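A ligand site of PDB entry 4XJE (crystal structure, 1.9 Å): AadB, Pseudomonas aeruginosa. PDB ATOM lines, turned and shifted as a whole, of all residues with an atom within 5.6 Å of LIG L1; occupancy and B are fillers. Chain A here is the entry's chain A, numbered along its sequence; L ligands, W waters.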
ATOM      1  N   GLY A  34      -3.112  21.189  38.371  1.00  0.00           N
ATOM      2  CA  GLY A  34      -4.055  21.436  37.300  1.00  0.00           C
ATOM      3  C   GLY A  34      -3.622  20.826  35.987  1.00  0.00           C
ATOM      4  O   GLY A  34      -2.570  20.185  35.896  1.00  0.00           O
ATOM      5  N   GLY A  35      -4.437  21.018  34.953  1.00  0.00           N
ATOM      6  CA  GLY A  35      -4.083  20.640  33.599  1.00  0.00           C
ATOM      7  C   GLY A  35      -3.755  19.173  33.420  1.00  0.00           C
ATOM      8  O   GLY A  35      -4.412  18.302  33.995  1.00  0.00           O
ATOM      9  N   GLY A  36      -2.732  18.911  32.623  1.00  0.00           N
ATOM     10  CA  GLY A  36      -2.352  17.545  32.272  1.00  0.00           C
ATOM     11  C   GLY A  36      -2.063  16.663  33.480  1.00  0.00           C
ATOM     12  O   GLY A  36      -2.506  15.521  33.530  1.00  0.00           O
ATOM     13  N   TRP A  37      -1.327  17.189  34.447  1.00  0.00           N
ATOM     14  CA  TRP A  37      -0.988  16.409  35.635  1.00  0.00           C
ATOM     15  C   TRP A  37      -2.211  16.144  36.512  1.00  0.00           C
ATOM     16  O   TRP A  37      -2.266  15.144  37.227  1.00  0.00           O
ATOM     17  CB  TRP A  37       0.104  17.100  36.458  1.00  0.00           C
ATOM     18  CG  TRP A  37       1.477  16.691  36.037  1.00  0.00           C
ATOM     19  CD1 TRP A  37       2.425  17.462  35.446  1.00  0.00           C
ATOM     20  CD2 TRP A  37       2.040  15.380  36.162  1.00  0.00           C
ATOM     21  NE1 TRP A  37       3.556  16.723  35.204  1.00  0.00           N
ATOM     22  CE2 TRP A  37       3.351  15.440  35.638  1.00  0.00           C
ATOM     23  CE3 TRP A  37       1.574  14.168  36.681  1.00  0.00           C
ATOM     24  CZ2 TRP A  37       4.185  14.331  35.608  1.00  0.00           C
ATOM     25  CZ3 TRP A  37       2.413  13.071  36.654  1.00  0.00           C
ATOM     26  CH2 TRP A  37       3.699  13.159  36.124  1.00  0.00           C
ATOM     27  N   ILE A  39      -5.219  15.536  35.309  1.00  0.00           N
ATOM     28  CA  ILE A  39      -5.849  14.408  34.648  1.00  0.00           C
ATOM     29  C   ILE A  39      -5.193  13.113  35.115  1.00  0.00           C
ATOM     30  O   ILE A  39      -5.874  12.207  35.586  1.00  0.00           O
ATOM     31  CB  ILE A  39      -5.767  14.528  33.108  1.00  0.00           C
ATOM     32  CG1 ILE A  39      -6.578  15.727  32.622  1.00  0.00           C
ATOM     33  CG2 ILE A  39      -6.259  13.246  32.426  1.00  0.00           C
ATOM     34  CD1 ILE A  39      -6.403  16.060  31.146  1.00  0.00           C
ATOM     35  N   HIS A  50       4.090  15.897  29.929  1.00  0.00           N
ATOM     36  CA  HIS A  50       3.444  17.161  30.219  1.00  0.00           C
ATOM     37  C   HIS A  50       4.492  18.271  30.048  1.00  0.00           C
ATOM     38  O   HIS A  50       5.633  18.124  30.468  1.00  0.00           O
ATOM     39  CB  HIS A  50       2.844  17.131  31.629  1.00  0.00           C
ATOM     40  CG  HIS A  50       2.004  15.925  31.901  1.00  0.00           C
ATOM     41  ND1 HIS A  50       0.735  15.744  31.375  1.00  0.00           N
ATOM     42  CD2 HIS A  50       2.243  14.825  32.654  1.00  0.00           C
ATOM     43  CE1 HIS A  50       0.243  14.595  31.782  1.00  0.00           C
ATOM     44  NE2 HIS A  50       1.134  14.018  32.565  1.00  0.00           N
ATOM     45  N   ASP A  51       4.084  19.368  29.400  1.00  0.00           N
ATOM     46  CA  ASP A  51       5.015  20.443  29.060  1.00  0.00           C
ATOM     47  C   ASP A  51       5.483  21.157  30.319  1.00  0.00           C
ATOM     48  O   ASP A  51       6.593  21.698  30.368  1.00  0.00           O
ATOM     49  CB  ASP A  51       4.376  21.472  28.127  1.00  0.00           C
ATOM     50  CG  ASP A  51       4.145  20.941  26.725  1.00  0.00           C
ATOM     51  OD1 ASP A  51       4.587  19.822  26.414  1.00  0.00           O
ATOM     52  OD2 ASP A  51       3.496  21.657  25.923  1.00  0.00           O
ATOM     53  N   ASP A  52       4.618  21.183  31.322  1.00  0.00           N
ATOM     54  CA  ASP A  52       4.880  21.948  32.527  1.00  0.00           C
ATOM     55  C   ASP A  52       4.055  21.423  33.686  1.00  0.00           C
ATOM     56  O   ASP A  52       3.330  20.429  33.551  1.00  0.00           O
ATOM     57  CB  ASP A  52       4.573  23.427  32.282  1.00  0.00           C
ATOM     58  CG  ASP A  52       3.175  23.654  31.722  1.00  0.00           C
ATOM     59  OD1 ASP A  52       2.335  22.745  31.784  1.00  0.00           O
ATOM     60  OD2 ASP A  52       2.920  24.776  31.220  1.00  0.00           O
ATOM     61  N   ASP A  54       1.120  22.667  36.219  1.00  0.00           N
ATOM     62  CA  ASP A  54       0.113  23.679  36.451  1.00  0.00           C
ATOM     63  C   ASP A  54      -0.296  23.675  37.912  1.00  0.00           C
ATOM     64  O   ASP A  54      -0.630  22.634  38.472  1.00  0.00           O
ATOM     65  CB  ASP A  54      -1.101  23.446  35.546  1.00  0.00           C
ATOM     66  CG  ASP A  54      -0.739  23.502  34.081  1.00  0.00           C
ATOM     67  OD1 ASP A  54      -0.335  24.594  33.610  1.00  0.00           O
ATOM     68  OD2 ASP A  54      -0.869  22.462  33.400  1.00  0.00           O
ATOM     69  N   ILE A 136     -10.870  21.215  34.475  1.00  0.00           N
ATOM     70  CA  ILE A 136      -9.943  20.683  33.475  1.00  0.00           C
ATOM     71  C   ILE A 136     -10.517  20.826  32.053  1.00  0.00           C
ATOM     72  O   ILE A 136      -9.843  21.333  31.151  1.00  0.00           O
ATOM     73  CB  ILE A 136      -9.629  19.196  33.770  1.00  0.00           C
ATOM     74  CG1 ILE A 136      -8.785  19.072  35.048  1.00  0.00           C
ATOM     75  CG2 ILE A 136      -8.895  18.533  32.606  1.00  0.00           C
ATOM     76  CD1 ILE A 136      -8.675  17.650  35.576  1.00  0.00           C
ATOM     77  N   ILE A 137     -11.744  20.349  31.879  1.00  0.00           N
ATOM     78  CA  ILE A 137     -12.439  20.414  30.589  1.00  0.00           C
ATOM     79  C   ILE A 137     -12.602  21.867  30.149  1.00  0.00           C
ATOM     80  O   ILE A 137     -12.373  22.201  28.986  1.00  0.00           O
ATOM     81  CB  ILE A 137     -13.829  19.735  30.676  1.00  0.00           C
ATOM     82  CG1 ILE A 137     -13.718  18.253  30.293  1.00  0.00           C
ATOM     83  CG2 ILE A 137     -14.855  20.437  29.772  1.00  0.00           C
ATOM     84  CD1 ILE A 137     -13.633  17.975  28.797  1.00  0.00           C
ATOM     85  N   ASP A 139     -10.940  24.502  30.402  1.00  0.00           N
ATOM     86  CA  ASP A 139      -9.803  25.146  29.755  1.00  0.00           C
ATOM     87  C   ASP A 139      -9.611  24.675  28.318  1.00  0.00           C
ATOM     88  O   ASP A 139      -9.002  25.382  27.512  1.00  0.00           O
ATOM     89  CB  ASP A 139      -8.526  24.930  30.563  1.00  0.00           C
ATOM     90  CG  ASP A 139      -8.384  25.916  31.711  1.00  0.00           C
ATOM     91  OD1 ASP A 139      -9.087  26.956  31.709  1.00  0.00           O
ATOM     92  OD2 ASP A 139      -7.554  25.673  32.615  1.00  0.00           O
ATOM     93  N   TYR A 140     -10.116  23.493  27.979  1.00  0.00           N
ATOM     94  CA  TYR A 140     -10.087  23.047  26.589  1.00  0.00           C
ATOM     95  C   TYR A 140     -11.040  23.855  25.706  1.00  0.00           C
ATOM     96  O   TYR A 140     -10.827  23.984  24.508  1.00  0.00           O
ATOM     97  CB  TYR A 140     -10.411  21.560  26.469  1.00  0.00           C
ATOM     98  CG  TYR A 140      -9.309  20.632  26.928  1.00  0.00           C
ATOM     99  CD1 TYR A 140      -8.189  20.428  26.150  1.00  0.00           C
ATOM    100  CD2 TYR A 140      -9.417  19.957  28.127  1.00  0.00           C
ATOM    101  CE1 TYR A 140      -7.179  19.572  26.569  1.00  0.00           C
ATOM    102  CE2 TYR A 140      -8.429  19.101  28.551  1.00  0.00           C
ATOM    103  CZ  TYR A 140      -7.317  18.913  27.781  1.00  0.00           C
ATOM    104  OH  TYR A 140      -6.330  18.062  28.218  1.00  0.00           O
ATOM    105  N   TYR A 142     -11.614  27.153  25.890  1.00  0.00           N
ATOM    106  CA  TYR A 142     -10.810  28.293  25.440  1.00  0.00           C
ATOM    107  C   TYR A 142      -9.885  27.889  24.311  1.00  0.00           C
ATOM    108  O   TYR A 142      -9.777  28.568  23.287  1.00  0.00           O
ATOM    109  CB  TYR A 142      -9.947  28.858  26.576  1.00  0.00           C
ATOM    110  CG  TYR A 142     -10.676  29.464  27.739  1.00  0.00           C
ATOM    111  CD1 TYR A 142     -11.255  30.722  27.665  1.00  0.00           C
ATOM    112  CD2 TYR A 142     -10.746  28.777  28.948  1.00  0.00           C
ATOM    113  CE1 TYR A 142     -11.899  31.278  28.759  1.00  0.00           C
ATOM    114  CE2 TYR A 142     -11.396  29.321  30.039  1.00  0.00           C
ATOM    115  CZ  TYR A 142     -11.971  30.568  29.938  1.00  0.00           C
ATOM    116  OH  TYR A 142     -12.605  31.080  31.035  1.00  0.00           O
ATOM    117  N   TYR A 143      -9.196  26.769  24.528  1.00  0.00           N
ATOM    118  CA  TYR A 143      -8.212  26.244  23.594  1.00  0.00           C
ATOM    119  C   TYR A 143      -8.850  26.038  22.227  1.00  0.00           C
ATOM    120  O   TYR A 143      -8.246  26.347  21.196  1.00  0.00           O
ATOM    121  CB  TYR A 143      -7.634  24.938  24.140  1.00  0.00           C
ATOM    122  CG  TYR A 143      -6.410  24.405  23.429  1.00  0.00           C
ATOM    123  CD1 TYR A 143      -5.627  25.209  22.605  1.00  0.00           C
ATOM    124  CD2 TYR A 143      -6.045  23.072  23.592  1.00  0.00           C
ATOM    125  CE1 TYR A 143      -4.515  24.689  21.967  1.00  0.00           C
ATOM    126  CE2 TYR A 143      -4.938  22.563  22.949  1.00  0.00           C
ATOM    127  CZ  TYR A 143      -4.179  23.372  22.143  1.00  0.00           C
ATOM    128  OH  TYR A 143      -3.079  22.856  21.510  1.00  0.00           O
ATOM    129  N   GLU A 146      -9.377  29.195  20.158  1.00  0.00           N
ATOM    130  CA  GLU A 146      -8.149  29.862  19.704  1.00  0.00           C
ATOM    131  C   GLU A 146      -7.382  29.032  18.680  1.00  0.00           C
ATOM    132  O   GLU A 146      -6.823  29.590  17.736  1.00  0.00           O
ATOM    133  CB  GLU A 146      -7.261  30.171  20.907  1.00  0.00           C
ATOM    134  CG  GLU A 146      -7.878  31.186  21.851  1.00  0.00           C
ATOM    135  CD  GLU A 146      -7.262  31.160  23.239  1.00  0.00           C
ATOM    136  OE1 GLU A 146      -7.908  31.654  24.182  1.00  0.00           O
ATOM    137  OE2 GLU A 146      -6.130  30.640  23.378  1.00  0.00           O
ATOM    138  N   VAL A 147      -7.349  27.726  18.876  1.00  0.00           N
ATOM    139  CA  VAL A 147      -6.650  26.824  17.973  1.00  0.00           C
ATOM    140  C   VAL A 147      -7.622  25.781  17.444  1.00  0.00           C
ATOM    141  O   VAL A 147      -8.253  25.072  18.233  1.00  0.00           O
ATOM    142  CB  VAL A 147      -5.476  26.107  18.663  1.00  0.00           C
ATOM    143  CG1 VAL A 147      -4.660  25.316  17.653  1.00  0.00           C
ATOM    144  CG2 VAL A 147      -4.604  27.108  19.396  1.00  0.00           C
ATOM    145  N   HIS A 156      -2.627  16.786  23.714  1.00  0.00           N
ATOM    146  CA  HIS A 156      -3.796  17.520  24.191  1.00  0.00           C
ATOM    147  C   HIS A 156      -5.099  16.863  23.766  1.00  0.00           C
ATOM    148  O   HIS A 156      -6.052  16.810  24.545  1.00  0.00           O
ATOM    149  CB  HIS A 156      -3.751  18.970  23.701  1.00  0.00           C
ATOM    150  CG  HIS A 156      -2.740  19.817  24.413  1.00  0.00           C
ATOM    151  ND1 HIS A 156      -2.675  19.899  25.783  1.00  0.00           N
ATOM    152  CD2 HIS A 156      -1.756  20.620  23.944  1.00  0.00           C
ATOM    153  CE1 HIS A 156      -1.694  20.708  26.131  1.00  0.00           C
ATOM    154  NE2 HIS A 156      -1.121  21.167  25.029  1.00  0.00           N
HETATM  155  P1  LIG L   1      -0.643  21.787  30.050  1.00  0.00           P
HETATM  156  O1  LIG L   1       0.003  22.803  30.971  1.00  0.00           O
HETATM  157  O2  LIG L   1       0.213  21.696  28.788  1.00  0.00           O
HETATM  158  O3  LIG L   1      -0.982  20.521  30.760  1.00  0.00           O
HETATM  159  O4  LIG L   1      -2.013  22.462  29.598  1.00  0.00           O
HETATM  160  C1  LIG L   1      -3.109  22.563  30.497  1.00  0.00           C
HETATM  161  C2  LIG L   1      -4.382  22.877  29.765  1.00  0.00           C
HETATM  162  O5  LIG L   1      -4.293  24.197  29.187  1.00  0.00           O
HETATM  163  C3  LIG L   1      -4.701  21.978  28.591  1.00  0.00           C
HETATM  164  O6  LIG L   1      -5.316  20.761  29.003  1.00  0.00           O
HETATM  165  C4  LIG L   1      -5.603  22.846  27.728  1.00  0.00           C
HETATM  166  O7  LIG L   1      -6.939  22.809  28.201  1.00  0.00           O
HETATM  167  C5  LIG L   1      -5.039  24.245  27.989  1.00  0.00           C
HETATM  168  N1  LIG L   1      -4.161  24.715  26.896  1.00  0.00           N
HETATM  169  C6  LIG L   1      -3.008  24.134  26.434  1.00  0.00           C
HETATM  170  N2  LIG L   1      -2.441  24.786  25.445  1.00  0.00           N
HETATM  171  C7  LIG L   1      -3.272  25.880  25.252  1.00  0.00           C
HETATM  172  C8  LIG L   1      -3.220  26.953  24.347  1.00  0.00           C
HETATM  173  N3  LIG L   1      -2.259  27.109  23.428  1.00  0.00           N
HETATM  174  N4  LIG L   1      -4.206  27.873  24.411  1.00  0.00           N
HETATM  175  C9  LIG L   1      -5.170  27.720  25.320  1.00  0.00           C
HETATM  176  N5  LIG L   1      -5.324  26.746  26.220  1.00  0.00           N
HETATM  177  C10 LIG L   1      -4.339  25.848  26.131  1.00  0.00           C
HETATM  178  C1  LG2 L   2      -7.777  29.829  30.728  1.00  0.00           C
HETATM  179  O1  LG2 L   2      -6.436  29.850  31.181  1.00  0.00           O
HETATM  180  C2  LG2 L   2      -7.907  30.780  29.550  1.00  0.00           C
HETATM  181  N1  LG2 L   2      -6.976  30.436  28.453  1.00  0.00           N
HETATM  182  C3  LG2 L   2      -7.685  32.206  30.042  1.00  0.00           C
HETATM  183  C4  LG2 L   2      -8.619  32.563  31.188  1.00  0.00           C
HETATM  184  O2  LG2 L   2      -8.294  33.864  31.666  1.00  0.00           O
HETATM  185  C5  LG2 L   2      -8.466  31.534  32.300  1.00  0.00           C
HETATM  186  O3  LG2 L   2      -8.657  30.199  31.768  1.00  0.00           O
HETATM  187  C6  LG2 L   2      -9.504  31.727  33.392  1.00  0.00           C
HETATM  188  N2  LG2 L   2      -9.395  30.739  34.474  1.00  0.00           N
HETATM  189  C7  LG2 L   2      -3.331  27.500  32.605  1.00  0.00           C
HETATM  190  N3  LG2 L   2      -2.419  26.428  33.014  1.00  0.00           N
HETATM  191  C8  LG2 L   2      -4.672  27.391  33.336  1.00  0.00           C
HETATM  192  C9  LG2 L   2      -5.606  28.534  32.935  1.00  0.00           C
HETATM  193  N4  LG2 L   2      -6.907  28.379  33.597  1.00  0.00           N
HETATM  194  C10 LG2 L   2      -5.784  28.600  31.415  1.00  0.00           C
HETATM  195  C11 LG2 L   2      -4.448  28.647  30.685  1.00  0.00           C
HETATM  196  O4  LG2 L   2      -4.668  28.607  29.280  1.00  0.00           O
HETATM  197  C12 LG2 L   2      -3.593  27.463  31.101  1.00  0.00           C
HETATM  198  O5  LG2 L   2      -2.334  27.542  30.434  1.00  0.00           O
HETATM  199  C13 LG2 L   2      -2.139  26.690  29.319  1.00  0.00           C
HETATM  200  C14 LG2 L   2      -0.776  26.030  29.442  1.00  0.00           C
HETATM  201  O6  LG2 L   2      -0.654  25.391  30.708  1.00  0.00           O
HETATM  202  C15 LG2 L   2       0.358  27.051  29.264  1.00  0.00           C
HETATM  203  N5  LG2 L   2       1.666  26.379  29.308  1.00  0.00           N
HETATM  204  C16 LG2 L   2       0.139  27.769  27.939  1.00  0.00           C
HETATM  205  O7  LG2 L   2       1.139  28.765  27.739  1.00  0.00           O
HETATM  206  C17 LG2 L   2      -1.236  28.431  27.982  1.00  0.00           C
HETATM  207  O8  LG2 L   2      -2.238  27.430  28.115  1.00  0.00           O
HETATM  208  C18 LG2 L   2      -1.564  29.228  26.743  1.00  0.00           C
HETATM  209  O9  LG2 L   2      -2.812  29.893  26.877  1.00  0.00           O
HETATM  210  O   HOH W   1      -7.282  27.415  28.181  1.00  0.00           O
HETATM  211  O   HOH W   2      -3.996  18.646  27.801  1.00  0.00           O
HETATM  212  O   HOH W   3       1.299  23.745  27.396  1.00  0.00           O
HETATM  213  O   HOH W   4       0.681  19.606  32.883  1.00  0.00           O
HETATM  214  O   HOH W   5      -7.152  21.305  31.228  1.00  0.00           O
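An oxygen (O6) of LIG L1 sits close to the side-chain hydroxyl (OH) of Tyr 140 (3.0 Å). A nitrogen (N3) of LG2 L2 lies within salt-bridge range of the side-chain carboxylate of Asp 54 (2.8 Å). OD1 of Asp 52 lies close to O1 of LIG L1, at 2.5 Å. OD2 of Asp 54 sits close to O1 of LIG L1. An oxygen (O7) of LIG L1 sits close to the backbone carbonyl oxygen (O) of Asp 139 (3.4 Å). A nitrogen (N5) of LG2 L2 is in salt-bridge range of the side-chain carboxylate (OD2) of Asp 52, at 2.8 Å. N of Gly 36 lies within hydrogen-bond range of O3 of LIG L1, at 3.0 Å. The backbone NH (N) of Tyr 140 sits at hydrogen-bond distance from an oxygen (O7) of LIG L1, 3.3 Å away. OD2 of Asp 139 lies within salt-bridge range of N4 of LG2 L2, 3.0 Å away.
An oxygen (O6) of LG2 L2 lies within hydrogen-bond range of an oxygen (O1) of LIG L1.
The backbone carbonyl oxygen of Asp 54 sits at hydrogen-bond distance from the backbone NH of Gly 34 (2.9 Å).
CA of Gly 35 touches C1 of LIG L1, at 3.8 Å. Tyr 143 touches LIG L1 (CD1 to C8, 3.4 Å). OE2 of Glu 146 touches N4 of LIG L1 (3.5 Å). CE1 of His 156 touches O2 of LIG L1 (3.4 Å). The nearest printed residue that does not touch LIG L1 is Asp 51 (4.2 Å).
Water W3 lies within hydrogen-bond range of an oxygen (O2) of LIG L1 (2.7 Å), a nitrogen (N5) of LG2 L2 (3.3 Å) and the side-chain carboxylate of Asp 51 (3.4 Å). Water W2 lies within hydrogen-bond range of OH of Tyr 140, ND1 of His 156 and O6 of LIG L1. Water W4 lies within hydrogen-bond range of an oxygen (O3) of LIG L1 (2.8 Å), the backbone carbonyl oxygen of Asp 52 (2.9 Å), the side-chain carboxylate of Asp 54 (3.3 Å) and the backbone NH of Gly 36 (3.5 Å). Water W1 lies within hydrogen-bond range of the backbone carbonyl oxygen (O) of Asp 139 (2.7 Å), a nitrogen (N5) of LIG L1 (2.9 Å) and a nitrogen (N1) of LG2 L2 (3.0 Å). Water W5 lies within hydrogen-bond range of the backbone carbonyl oxygen (O) of Ile 136 and an oxygen (O6) of LIG L1.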
